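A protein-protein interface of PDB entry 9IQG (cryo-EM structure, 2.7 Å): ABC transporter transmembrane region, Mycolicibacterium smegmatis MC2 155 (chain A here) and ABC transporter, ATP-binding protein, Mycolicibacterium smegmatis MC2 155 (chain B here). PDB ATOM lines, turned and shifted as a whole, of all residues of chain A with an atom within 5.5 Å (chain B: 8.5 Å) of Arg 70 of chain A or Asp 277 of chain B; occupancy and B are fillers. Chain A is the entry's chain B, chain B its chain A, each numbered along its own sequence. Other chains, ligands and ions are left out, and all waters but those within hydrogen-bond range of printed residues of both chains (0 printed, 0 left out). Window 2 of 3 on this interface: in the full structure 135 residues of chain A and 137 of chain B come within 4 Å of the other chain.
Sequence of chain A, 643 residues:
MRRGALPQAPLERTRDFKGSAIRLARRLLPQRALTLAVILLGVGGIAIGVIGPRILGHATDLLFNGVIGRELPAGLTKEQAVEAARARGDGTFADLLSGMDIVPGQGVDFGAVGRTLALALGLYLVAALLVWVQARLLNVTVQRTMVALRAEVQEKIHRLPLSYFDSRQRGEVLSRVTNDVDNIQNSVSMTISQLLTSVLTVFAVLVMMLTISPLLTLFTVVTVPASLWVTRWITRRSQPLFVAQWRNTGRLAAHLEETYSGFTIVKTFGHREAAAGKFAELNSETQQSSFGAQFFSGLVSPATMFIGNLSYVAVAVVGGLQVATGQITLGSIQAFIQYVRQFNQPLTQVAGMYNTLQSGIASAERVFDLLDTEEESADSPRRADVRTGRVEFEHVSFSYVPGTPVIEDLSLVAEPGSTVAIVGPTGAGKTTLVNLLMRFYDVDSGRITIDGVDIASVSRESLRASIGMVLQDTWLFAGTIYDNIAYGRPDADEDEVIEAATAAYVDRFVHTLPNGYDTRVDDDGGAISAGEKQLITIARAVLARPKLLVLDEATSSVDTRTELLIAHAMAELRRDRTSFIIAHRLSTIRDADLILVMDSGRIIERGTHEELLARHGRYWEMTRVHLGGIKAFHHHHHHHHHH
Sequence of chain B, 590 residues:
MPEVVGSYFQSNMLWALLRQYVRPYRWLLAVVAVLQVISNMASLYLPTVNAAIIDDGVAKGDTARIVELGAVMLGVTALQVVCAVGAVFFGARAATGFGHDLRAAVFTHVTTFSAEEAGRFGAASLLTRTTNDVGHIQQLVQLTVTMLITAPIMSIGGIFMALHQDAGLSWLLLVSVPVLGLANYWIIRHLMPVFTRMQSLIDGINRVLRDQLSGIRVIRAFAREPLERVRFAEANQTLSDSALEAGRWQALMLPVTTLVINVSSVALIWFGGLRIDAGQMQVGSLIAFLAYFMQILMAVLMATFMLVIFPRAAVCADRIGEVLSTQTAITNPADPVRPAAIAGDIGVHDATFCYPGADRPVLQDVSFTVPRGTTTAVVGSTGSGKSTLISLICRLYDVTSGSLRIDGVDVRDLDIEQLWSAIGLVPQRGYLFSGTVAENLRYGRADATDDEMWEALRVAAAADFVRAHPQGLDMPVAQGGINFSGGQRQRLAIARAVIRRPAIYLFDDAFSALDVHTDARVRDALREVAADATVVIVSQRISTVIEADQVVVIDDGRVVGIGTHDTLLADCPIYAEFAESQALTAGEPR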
ATOM      1  N   ASN A  65      20.531 -19.801 -22.453  1.00  0.00           N
ATOM      2  CA  ASN A  65      19.250 -20.464 -22.648  1.00  0.00           C
ATOM      3  C   ASN A  65      19.191 -21.140 -24.006  1.00  0.00           C
ATOM      4  O   ASN A  65      18.792 -22.305 -24.110  1.00  0.00           O
ATOM      5  CB  ASN A  65      18.113 -19.452 -22.514  1.00  0.00           C
ATOM      6  CG  ASN A  65      17.817 -19.096 -21.078  1.00  0.00           C
ATOM      7  OD1 ASN A  65      18.103 -19.866 -20.168  1.00  0.00           O
ATOM      8  ND2 ASN A  65      17.241 -17.920 -20.867  1.00  0.00           N
ATOM      9  N   GLY A  66      19.596 -20.429 -25.060  1.00  0.00           N
ATOM     10  CA  GLY A  66      19.583 -21.029 -26.383  1.00  0.00           C
ATOM     11  C   GLY A  66      20.504 -22.229 -26.483  1.00  0.00           C
ATOM     12  O   GLY A  66      20.128 -23.274 -27.019  1.00  0.00           O
ATOM     13  N   VAL A  67      21.721 -22.099 -25.950  1.00  0.00           N
ATOM     14  CA  VAL A  67      22.702 -23.174 -26.064  1.00  0.00           C
ATOM     15  C   VAL A  67      22.238 -24.411 -25.305  1.00  0.00           C
ATOM     16  O   VAL A  67      22.384 -25.541 -25.787  1.00  0.00           O
ATOM     17  CB  VAL A  67      24.079 -22.686 -25.580  1.00  0.00           C
ATOM     18  CG1 VAL A  67      25.017 -23.857 -25.351  1.00  0.00           C
ATOM     19  CG2 VAL A  67      24.666 -21.726 -26.593  1.00  0.00           C
ATOM     20  N   ILE A  68      21.675 -24.224 -24.110  1.00  0.00           N
ATOM     21  CA  ILE A  68      21.211 -25.367 -23.332  1.00  0.00           C
ATOM     22  C   ILE A  68      19.983 -26.001 -23.978  1.00  0.00           C
ATOM     23  O   ILE A  68      19.889 -27.230 -24.083  1.00  0.00           O
ATOM     24  CB  ILE A  68      20.935 -24.949 -21.878  1.00  0.00           C
ATOM     25  CG1 ILE A  68      22.244 -24.612 -21.166  1.00  0.00           C
ATOM     26  CG2 ILE A  68      20.212 -26.053 -21.142  1.00  0.00           C
ATOM     27  CD1 ILE A  68      23.118 -25.811 -20.896  1.00  0.00           C
ATOM     28  N   GLY A  69      19.028 -25.183 -24.430  1.00  0.00           N
ATOM     29  CA  GLY A  69      17.805 -25.723 -24.992  1.00  0.00           C
ATOM     30  C   GLY A  69      17.953 -26.322 -26.372  1.00  0.00           C
ATOM     31  O   GLY A  69      17.087 -27.094 -26.792  1.00  0.00           O
ATOM     32  N   ARG A  70      19.025 -25.980 -27.089  1.00  0.00           N
ATOM     33  CA  ARG A  70      19.240 -26.565 -28.408  1.00  0.00           C
ATOM     34  C   ARG A  70      19.471 -28.068 -28.316  1.00  0.00           C
ATOM     35  O   ARG A  70      18.985 -28.832 -29.159  1.00  0.00           O
ATOM     36  CB  ARG A  70      20.421 -25.880 -29.093  1.00  0.00           C
ATOM     37  CG  ARG A  70      20.350 -25.887 -30.606  1.00  0.00           C
ATOM     38  CD  ARG A  70      21.677 -25.474 -31.215  1.00  0.00           C
ATOM     39  NE  ARG A  70      22.801 -25.820 -30.354  1.00  0.00           N
ATOM     40  CZ  ARG A  70      23.857 -25.045 -30.153  1.00  0.00           C
ATOM     41  NH1 ARG A  70      23.971 -23.867 -30.743  1.00  0.00           N
ATOM     42  NH2 ARG A  70      24.824 -25.462 -29.342  1.00  0.00           N
ATOM     43  N   GLU A  71      20.209 -28.514 -27.299  1.00  0.00           N
ATOM     44  CA  GLU A  71      20.578 -29.918 -27.180  1.00  0.00           C
ATOM     45  C   GLU A  71      19.459 -30.797 -26.637  1.00  0.00           C
ATOM     46  O   GLU A  71      19.579 -32.026 -26.695  1.00  0.00           O
ATOM     47  CB  GLU A  71      21.814 -30.060 -26.289  1.00  0.00           C
ATOM     48  CG  GLU A  71      23.130 -29.893 -27.029  1.00  0.00           C
ATOM     49  CD  GLU A  71      23.791 -31.219 -27.353  1.00  0.00           C
ATOM     50  OE1 GLU A  71      24.897 -31.207 -27.932  1.00  0.00           O
ATOM     51  OE2 GLU A  71      23.202 -32.272 -27.030  1.00  0.00           O
ATOM     52  N   LEU A  72      18.387 -30.214 -26.112  1.00  0.00           N
ATOM     53  CA  LEU A  72      17.314 -31.071 -25.633  1.00  0.00           C
ATOM     54  C   LEU A  72      16.350 -31.413 -26.767  1.00  0.00           C
ATOM     55  O   LEU A  72      16.225 -30.653 -27.732  1.00  0.00           O
ATOM     56  CB  LEU A  72      16.553 -30.388 -24.500  1.00  0.00           C
ATOM     57  CG  LEU A  72      17.352 -30.155 -23.219  1.00  0.00           C
ATOM     58  CD1 LEU A  72      16.545 -29.341 -22.229  1.00  0.00           C
ATOM     59  CD2 LEU A  72      17.781 -31.477 -22.607  1.00  0.00           C
ATOM     60  N   VAL A 103      13.272 -23.121 -23.918  1.00  0.00           N
ATOM     61  CA  VAL A 103      12.333 -23.783 -24.819  1.00  0.00           C
ATOM     62  C   VAL A 103      13.117 -24.813 -25.624  1.00  0.00           C
ATOM     63  O   VAL A 103      13.924 -24.435 -26.487  1.00  0.00           O
ATOM     64  CB  VAL A 103      11.623 -22.773 -25.735  1.00  0.00           C
ATOM     65  CG1 VAL A 103      10.455 -23.437 -26.447  1.00  0.00           C
ATOM     66  CG2 VAL A 103      11.156 -21.568 -24.938  1.00  0.00           C
ATOM     67  N   PRO A 104      12.928 -26.107 -25.374  1.00  0.00           N
ATOM     68  CA  PRO A 104      13.776 -27.116 -26.021  1.00  0.00           C
ATOM     69  C   PRO A 104      13.662 -27.076 -27.538  1.00  0.00           C
ATOM     70  O   PRO A 104      12.584 -26.860 -28.096  1.00  0.00           O
ATOM     71  CB  PRO A 104      13.246 -28.438 -25.454  1.00  0.00           C
ATOM     72  CG  PRO A 104      12.585 -28.060 -24.169  1.00  0.00           C
ATOM     73  CD  PRO A 104      11.986 -26.710 -24.419  1.00  0.00           C
ATOM     74  N   GLY A 105      14.797 -27.285 -28.203  1.00  0.00           N
ATOM     75  CA  GLY A 105      14.844 -27.304 -29.650  1.00  0.00           C
ATOM     76  C   GLY A 105      14.784 -25.951 -30.322  1.00  0.00           C
ATOM     77  O   GLY A 105      14.503 -25.891 -31.524  1.00  0.00           O
ATOM     78  N   GLN A 106      15.029 -24.863 -29.593  1.00  0.00           N
ATOM     79  CA  GLN A 106      14.941 -23.531 -30.179  1.00  0.00           C
ATOM     80  C   GLN A 106      16.298 -22.997 -30.622  1.00  0.00           C
ATOM     81  O   GLN A 106      16.433 -22.493 -31.741  1.00  0.00           O
ATOM     82  CB  GLN A 106      14.293 -22.562 -29.186  1.00  0.00           C
ATOM     83  CG  GLN A 106      12.781 -22.662 -29.132  1.00  0.00           C
ATOM     84  CD  GLN A 106      12.125 -22.300 -30.448  1.00  0.00           C
ATOM     85  OE1 GLN A 106      12.545 -21.363 -31.128  1.00  0.00           O
ATOM     86  NE2 GLN A 106      11.088 -23.042 -30.817  1.00  0.00           N
ATOM     87  N   GLY A 107      17.306 -23.097 -29.766  1.00  0.00           N
ATOM     88  CA  GLY A 107      18.597 -22.525 -30.074  1.00  0.00           C
ATOM     89  C   GLY A 107      18.668 -21.054 -29.709  1.00  0.00           C
ATOM     90  O   GLY A 107      17.750 -20.471 -29.127  1.00  0.00           O
ATOM     91  N   VAL A 108      19.793 -20.448 -30.067  1.00  0.00           N
ATOM     92  CA  VAL A 108      20.058 -19.059 -29.710  1.00  0.00           C
ATOM     93  C   VAL A 108      19.377 -18.139 -30.714  1.00  0.00           C
ATOM     94  O   VAL A 108      19.564 -18.276 -31.930  1.00  0.00           O
ATOM     95  CB  VAL A 108      21.569 -18.789 -29.650  1.00  0.00           C
ATOM     96  CG1 VAL A 108      21.831 -17.330 -29.326  1.00  0.00           C
ATOM     97  CG2 VAL A 108      22.226 -19.690 -28.623  1.00  0.00           C
ATOM     98  N   PHE A 110      19.716 -14.869 -32.130  1.00  0.00           N
ATOM     99  CA  PHE A 110      20.737 -13.831 -32.197  1.00  0.00           C
ATOM    100  C   PHE A 110      20.150 -12.446 -32.435  1.00  0.00           C
ATOM    101  O   PHE A 110      20.841 -11.451 -32.201  1.00  0.00           O
ATOM    102  CB  PHE A 110      21.758 -14.166 -33.282  1.00  0.00           C
ATOM    103  CG  PHE A 110      22.911 -14.986 -32.786  1.00  0.00           C
ATOM    104  CD1 PHE A 110      23.939 -14.396 -32.073  1.00  0.00           C
ATOM    105  CD2 PHE A 110      22.958 -16.348 -33.019  1.00  0.00           C
ATOM    106  CE1 PHE A 110      24.996 -15.149 -31.610  1.00  0.00           C
ATOM    107  CE2 PHE A 110      24.014 -17.105 -32.558  1.00  0.00           C
ATOM    108  CZ  PHE A 110      25.034 -16.505 -31.853  1.00  0.00           C
ATOM    109  N   TRP B 270      29.004 -10.137 -28.041  1.00  0.00           N
ATOM    110  CA  TRP B 270      28.545 -10.512 -29.378  1.00  0.00           C
ATOM    111  C   TRP B 270      29.380 -11.650 -29.965  1.00  0.00           C
ATOM    112  O   TRP B 270      28.845 -12.690 -30.376  1.00  0.00           O
ATOM    113  CB  TRP B 270      28.578  -9.289 -30.296  1.00  0.00           C
ATOM    114  CG  TRP B 270      28.146  -9.568 -31.702  1.00  0.00           C
ATOM    115  CD1 TRP B 270      28.910  -9.479 -32.825  1.00  0.00           C
ATOM    116  CD2 TRP B 270      26.844  -9.982 -32.135  1.00  0.00           C
ATOM    117  NE1 TRP B 270      28.169  -9.811 -33.931  1.00  0.00           N
ATOM    118  CE2 TRP B 270      26.896 -10.125 -33.533  1.00  0.00           C
ATOM    119  CE3 TRP B 270      25.642 -10.246 -31.474  1.00  0.00           C
ATOM    120  CZ2 TRP B 270      25.794 -10.520 -34.283  1.00  0.00           C
ATOM    121  CZ3 TRP B 270      24.550 -10.639 -32.221  1.00  0.00           C
ATOM    122  CH2 TRP B 270      24.633 -10.771 -33.610  1.00  0.00           C
ATOM    123  N   PHE B 271      30.703 -11.483 -29.990  1.00  0.00           N
ATOM    124  CA  PHE B 271      31.549 -12.470 -30.653  1.00  0.00           C
ATOM    125  C   PHE B 271      31.689 -13.737 -29.817  1.00  0.00           C
ATOM    126  O   PHE B 271      31.777 -14.842 -30.368  1.00  0.00           O
ATOM    127  CB  PHE B 271      32.913 -11.859 -30.967  1.00  0.00           C
ATOM    128  CG  PHE B 271      32.872 -10.831 -32.063  1.00  0.00           C
ATOM    129  CD1 PHE B 271      32.556 -11.195 -33.361  1.00  0.00           C
ATOM    130  CD2 PHE B 271      33.138  -9.500 -31.797  1.00  0.00           C
ATOM    131  CE1 PHE B 271      32.511 -10.254 -34.369  1.00  0.00           C
ATOM    132  CE2 PHE B 271      33.094  -8.555 -32.802  1.00  0.00           C
ATOM    133  CZ  PHE B 271      32.781  -8.934 -34.090  1.00  0.00           C
ATOM    134  N   GLY B 272      31.695 -13.610 -28.491  1.00  0.00           N
ATOM    135  CA  GLY B 272      31.675 -14.785 -27.646  1.00  0.00           C
ATOM    136  C   GLY B 272      30.387 -15.568 -27.777  1.00  0.00           C
ATOM    137  O   GLY B 272      30.397 -16.792 -27.716  1.00  0.00           O
ATOM    138  N   GLY B 273      29.262 -14.877 -27.963  1.00  0.00           N
ATOM    139  CA  GLY B 273      28.024 -15.582 -28.241  1.00  0.00           C
ATOM    140  C   GLY B 273      28.050 -16.282 -29.584  1.00  0.00           C
ATOM    141  O   GLY B 273      27.528 -17.391 -29.727  1.00  0.00           O
ATOM    142  N   LEU B 274      28.657 -15.645 -30.586  1.00  0.00           N
ATOM    143  CA  LEU B 274      28.826 -16.310 -31.875  1.00  0.00           C
ATOM    144  C   LEU B 274      29.672 -17.571 -31.737  1.00  0.00           C
ATOM    145  O   LEU B 274      29.382 -18.594 -32.365  1.00  0.00           O
ATOM    146  CB  LEU B 274      29.451 -15.351 -32.887  1.00  0.00           C
ATOM    147  CG  LEU B 274      28.507 -14.330 -33.524  1.00  0.00           C
ATOM    148  CD1 LEU B 274      29.290 -13.293 -34.301  1.00  0.00           C
ATOM    149  CD2 LEU B 274      27.500 -15.024 -34.420  1.00  0.00           C
ATOM    150  N   ARG B 275      30.725 -17.513 -30.921  1.00  0.00           N
ATOM    151  CA  ARG B 275      31.576 -18.683 -30.715  1.00  0.00           C
ATOM    152  C   ARG B 275      30.926 -19.729 -29.813  1.00  0.00           C
ATOM    153  O   ARG B 275      31.237 -20.918 -29.931  1.00  0.00           O
ATOM    154  CB  ARG B 275      32.921 -18.257 -30.129  1.00  0.00           C
ATOM    155  CG  ARG B 275      33.848 -17.610 -31.136  1.00  0.00           C
ATOM    156  CD  ARG B 275      35.159 -17.197 -30.498  1.00  0.00           C
ATOM    157  NE  ARG B 275      35.908 -18.340 -29.993  1.00  0.00           N
ATOM    158  CZ  ARG B 275      36.615 -19.165 -30.753  1.00  0.00           C
ATOM    159  NH1 ARG B 275      36.687 -19.007 -32.063  1.00  0.00           N
ATOM    160  NH2 ARG B 275      37.270 -20.171 -30.182  1.00  0.00           N
ATOM    161  N   ILE B 276      30.044 -19.309 -28.907  1.00  0.00           N
ATOM    162  CA  ILE B 276      29.382 -20.230 -27.989  1.00  0.00           C
ATOM    163  C   ILE B 276      28.230 -20.945 -28.682  1.00  0.00           C
ATOM    164  O   ILE B 276      27.911 -22.091 -28.341  1.00  0.00           O
ATOM    165  CB  ILE B 276      28.916 -19.465 -26.735  1.00  0.00           C
ATOM    166  CG1 ILE B 276      30.091 -19.200 -25.797  1.00  0.00           C
ATOM    167  CG2 ILE B 276      27.848 -20.225 -25.977  1.00  0.00           C
ATOM    168  CD1 ILE B 276      29.804 -18.132 -24.769  1.00  0.00           C
ATOM    169  N   ASP B 277      27.598 -20.298 -29.664  1.00  0.00           N
ATOM    170  CA  ASP B 277      26.601 -20.986 -30.474  1.00  0.00           C
ATOM    171  C   ASP B 277      27.201 -22.224 -31.129  1.00  0.00           C
ATOM    172  O   ASP B 277      26.544 -23.267 -31.230  1.00  0.00           O
ATOM    173  CB  ASP B 277      26.034 -20.035 -31.528  1.00  0.00           C
ATOM    174  CG  ASP B 277      24.899 -20.651 -32.318  1.00  0.00           C
ATOM    175  OD1 ASP B 277      23.928 -21.126 -31.693  1.00  0.00           O
ATOM    176  OD2 ASP B 277      24.976 -20.661 -33.565  1.00  0.00           O
ATOM    177  N   ALA B 278      28.451 -22.128 -31.572  1.00  0.00           N
ATOM    178  CA  ALA B 278      29.215 -23.293 -31.976  1.00  0.00           C
ATOM    179  C   ALA B 278      29.917 -23.906 -30.764  1.00  0.00           C
ATOM    180  O   ALA B 278      29.916 -23.351 -29.663  1.00  0.00           O
ATOM    181  CB  ALA B 278      30.230 -22.919 -33.054  1.00  0.00           C
ATOM    182  N   GLY B 279      30.525 -25.066 -30.972  1.00  0.00           N
ATOM    183  CA  GLY B 279      31.233 -25.721 -29.889  1.00  0.00           C
ATOM    184  C   GLY B 279      32.651 -25.218 -29.724  1.00  0.00           C
ATOM    185  O   GLY B 279      33.593 -26.012 -29.652  1.00  0.00           O
ATOM    186  N   GLN B 280      32.819 -23.896 -29.660  1.00  0.00           N
ATOM    187  CA  GLN B 280      34.141 -23.290 -29.635  1.00  0.00           C
ATOM    188  C   GLN B 280      34.449 -22.528 -28.355  1.00  0.00           C
ATOM    189  O   GLN B 280      35.614 -22.186 -28.129  1.00  0.00           O
ATOM    190  CB  GLN B 280      34.310 -22.345 -30.834  1.00  0.00           C
ATOM    191  CG  GLN B 280      34.225 -23.038 -32.182  1.00  0.00           C
ATOM    192  CD  GLN B 280      34.154 -22.061 -33.339  1.00  0.00           C
ATOM    193  OE1 GLN B 280      34.314 -20.855 -33.160  1.00  0.00           O
ATOM    194  NE2 GLN B 280      33.910 -22.580 -34.537  1.00  0.00           N
ATOM    195  N   MET B 281      33.454 -22.252 -27.516  1.00  0.00           N
ATOM    196  CA  MET B 281      33.681 -21.435 -26.336  1.00  0.00           C
ATOM    197  C   MET B 281      32.670 -21.801 -25.260  1.00  0.00           C
ATOM    198  O   MET B 281      31.584 -22.307 -25.555  1.00  0.00           O
ATOM    199  CB  MET B 281      33.592 -19.944 -26.679  1.00  0.00           C
ATOM    200  CG  MET B 281      34.280 -19.025 -25.693  1.00  0.00           C
ATOM    201  SD  MET B 281      33.982 -17.292 -26.077  1.00  0.00           S
ATOM    202  CE  MET B 281      33.242 -16.730 -24.553  1.00  0.00           C
ATOM    203  N   GLN B 282      33.042 -21.541 -24.012  1.00  0.00           N
ATOM    204  CA  GLN B 282      32.194 -21.788 -22.858  1.00  0.00           C
ATOM    205  C   GLN B 282      31.677 -20.468 -22.303  1.00  0.00           C
ATOM    206  O   GLN B 282      32.229 -19.398 -22.571  1.00  0.00           O
ATOM    207  CB  GLN B 282      32.954 -22.559 -21.774  1.00  0.00           C
ATOM    208  CG  GLN B 282      33.602 -23.838 -22.271  1.00  0.00           C
ATOM    209  CD  GLN B 282      32.748 -25.062 -22.015  1.00  0.00           C
ATOM    210  OE1 GLN B 282      31.860 -25.389 -22.803  1.00  0.00           O
ATOM    211  NE2 GLN B 282      33.017 -25.750 -20.914  1.00  0.00           N
ATOM    212  N   VAL B 283      30.602 -20.555 -21.519  1.00  0.00           N
ATOM    213  CA  VAL B 283      29.914 -19.349 -21.071  1.00  0.00           C
ATOM    214  C   VAL B 283      30.752 -18.585 -20.051  1.00  0.00           C
ATOM    215  O   VAL B 283      30.774 -17.349 -20.054  1.00  0.00           O
ATOM    216  CB  VAL B 283      28.525 -19.701 -20.518  1.00  0.00           C
ATOM    217  CG1 VAL B 283      27.645 -18.466 -20.496  1.00  0.00           C
ATOM    218  CG2 VAL B 283      27.891 -20.795 -21.353  1.00  0.00           C
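Of the 14 printed residues of chain B, 5 touch a printed residue of chain A.
Hydrophobic or aromatic side chains of chain B that line the printed part of chain A: Trp 270, Leu 274 and Ile 276.
Along chain B the printed residues that touch a printed residue of chain A span positions 270 to 277.
Among the printed residues, 7 pairs touch across the chains.
Of chain B, only Asp 277 (2.7 Å) comes within 4 Å of Arg 70 of chain A.
Val 103 of chain A touches none of the printed residues of chain B.
Gly 272 of chain B touches none of the printed residues of chain A.
Of the printed residues of chain A, Gly 273 of chain B touches Phe 110 (3.4 Å).
Of the printed residues of chain A, Ile 276 of chain B touches Val 67 (3.6 Å).
Asp 277 of chain B touches just these residues of chain A: Arg 70 (2.7 Å), Val 108 (3.8 Å) and Phe 110 (3.7 Å).
The nearest residue of chain B that does not touch Arg 70 of chain A is Ile 276 of chain B (4.7 Å).
The nearest residue of chain A that does not touch Asp 277 of chain B is Val 67 of chain A (4.4 Å).
Among the printed residues, merely in contact across the chains: Phe 110 of chain A with Gly 273 of chain B, Val 67 of chain A with Ile 276 of chain B, Phe 110 of chain A with Asp 277 of chain B, Phe 110 of chain A with Leu 274 of chain B, Val 108 of chain A with Asp 277 of chain B and Phe 110 of chain A with Trp 270 of chain B.
OD1 of Asp 277 of chain B lies within salt-bridge range of NH1 of Arg 70 of chain A, at 2.9 Å.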
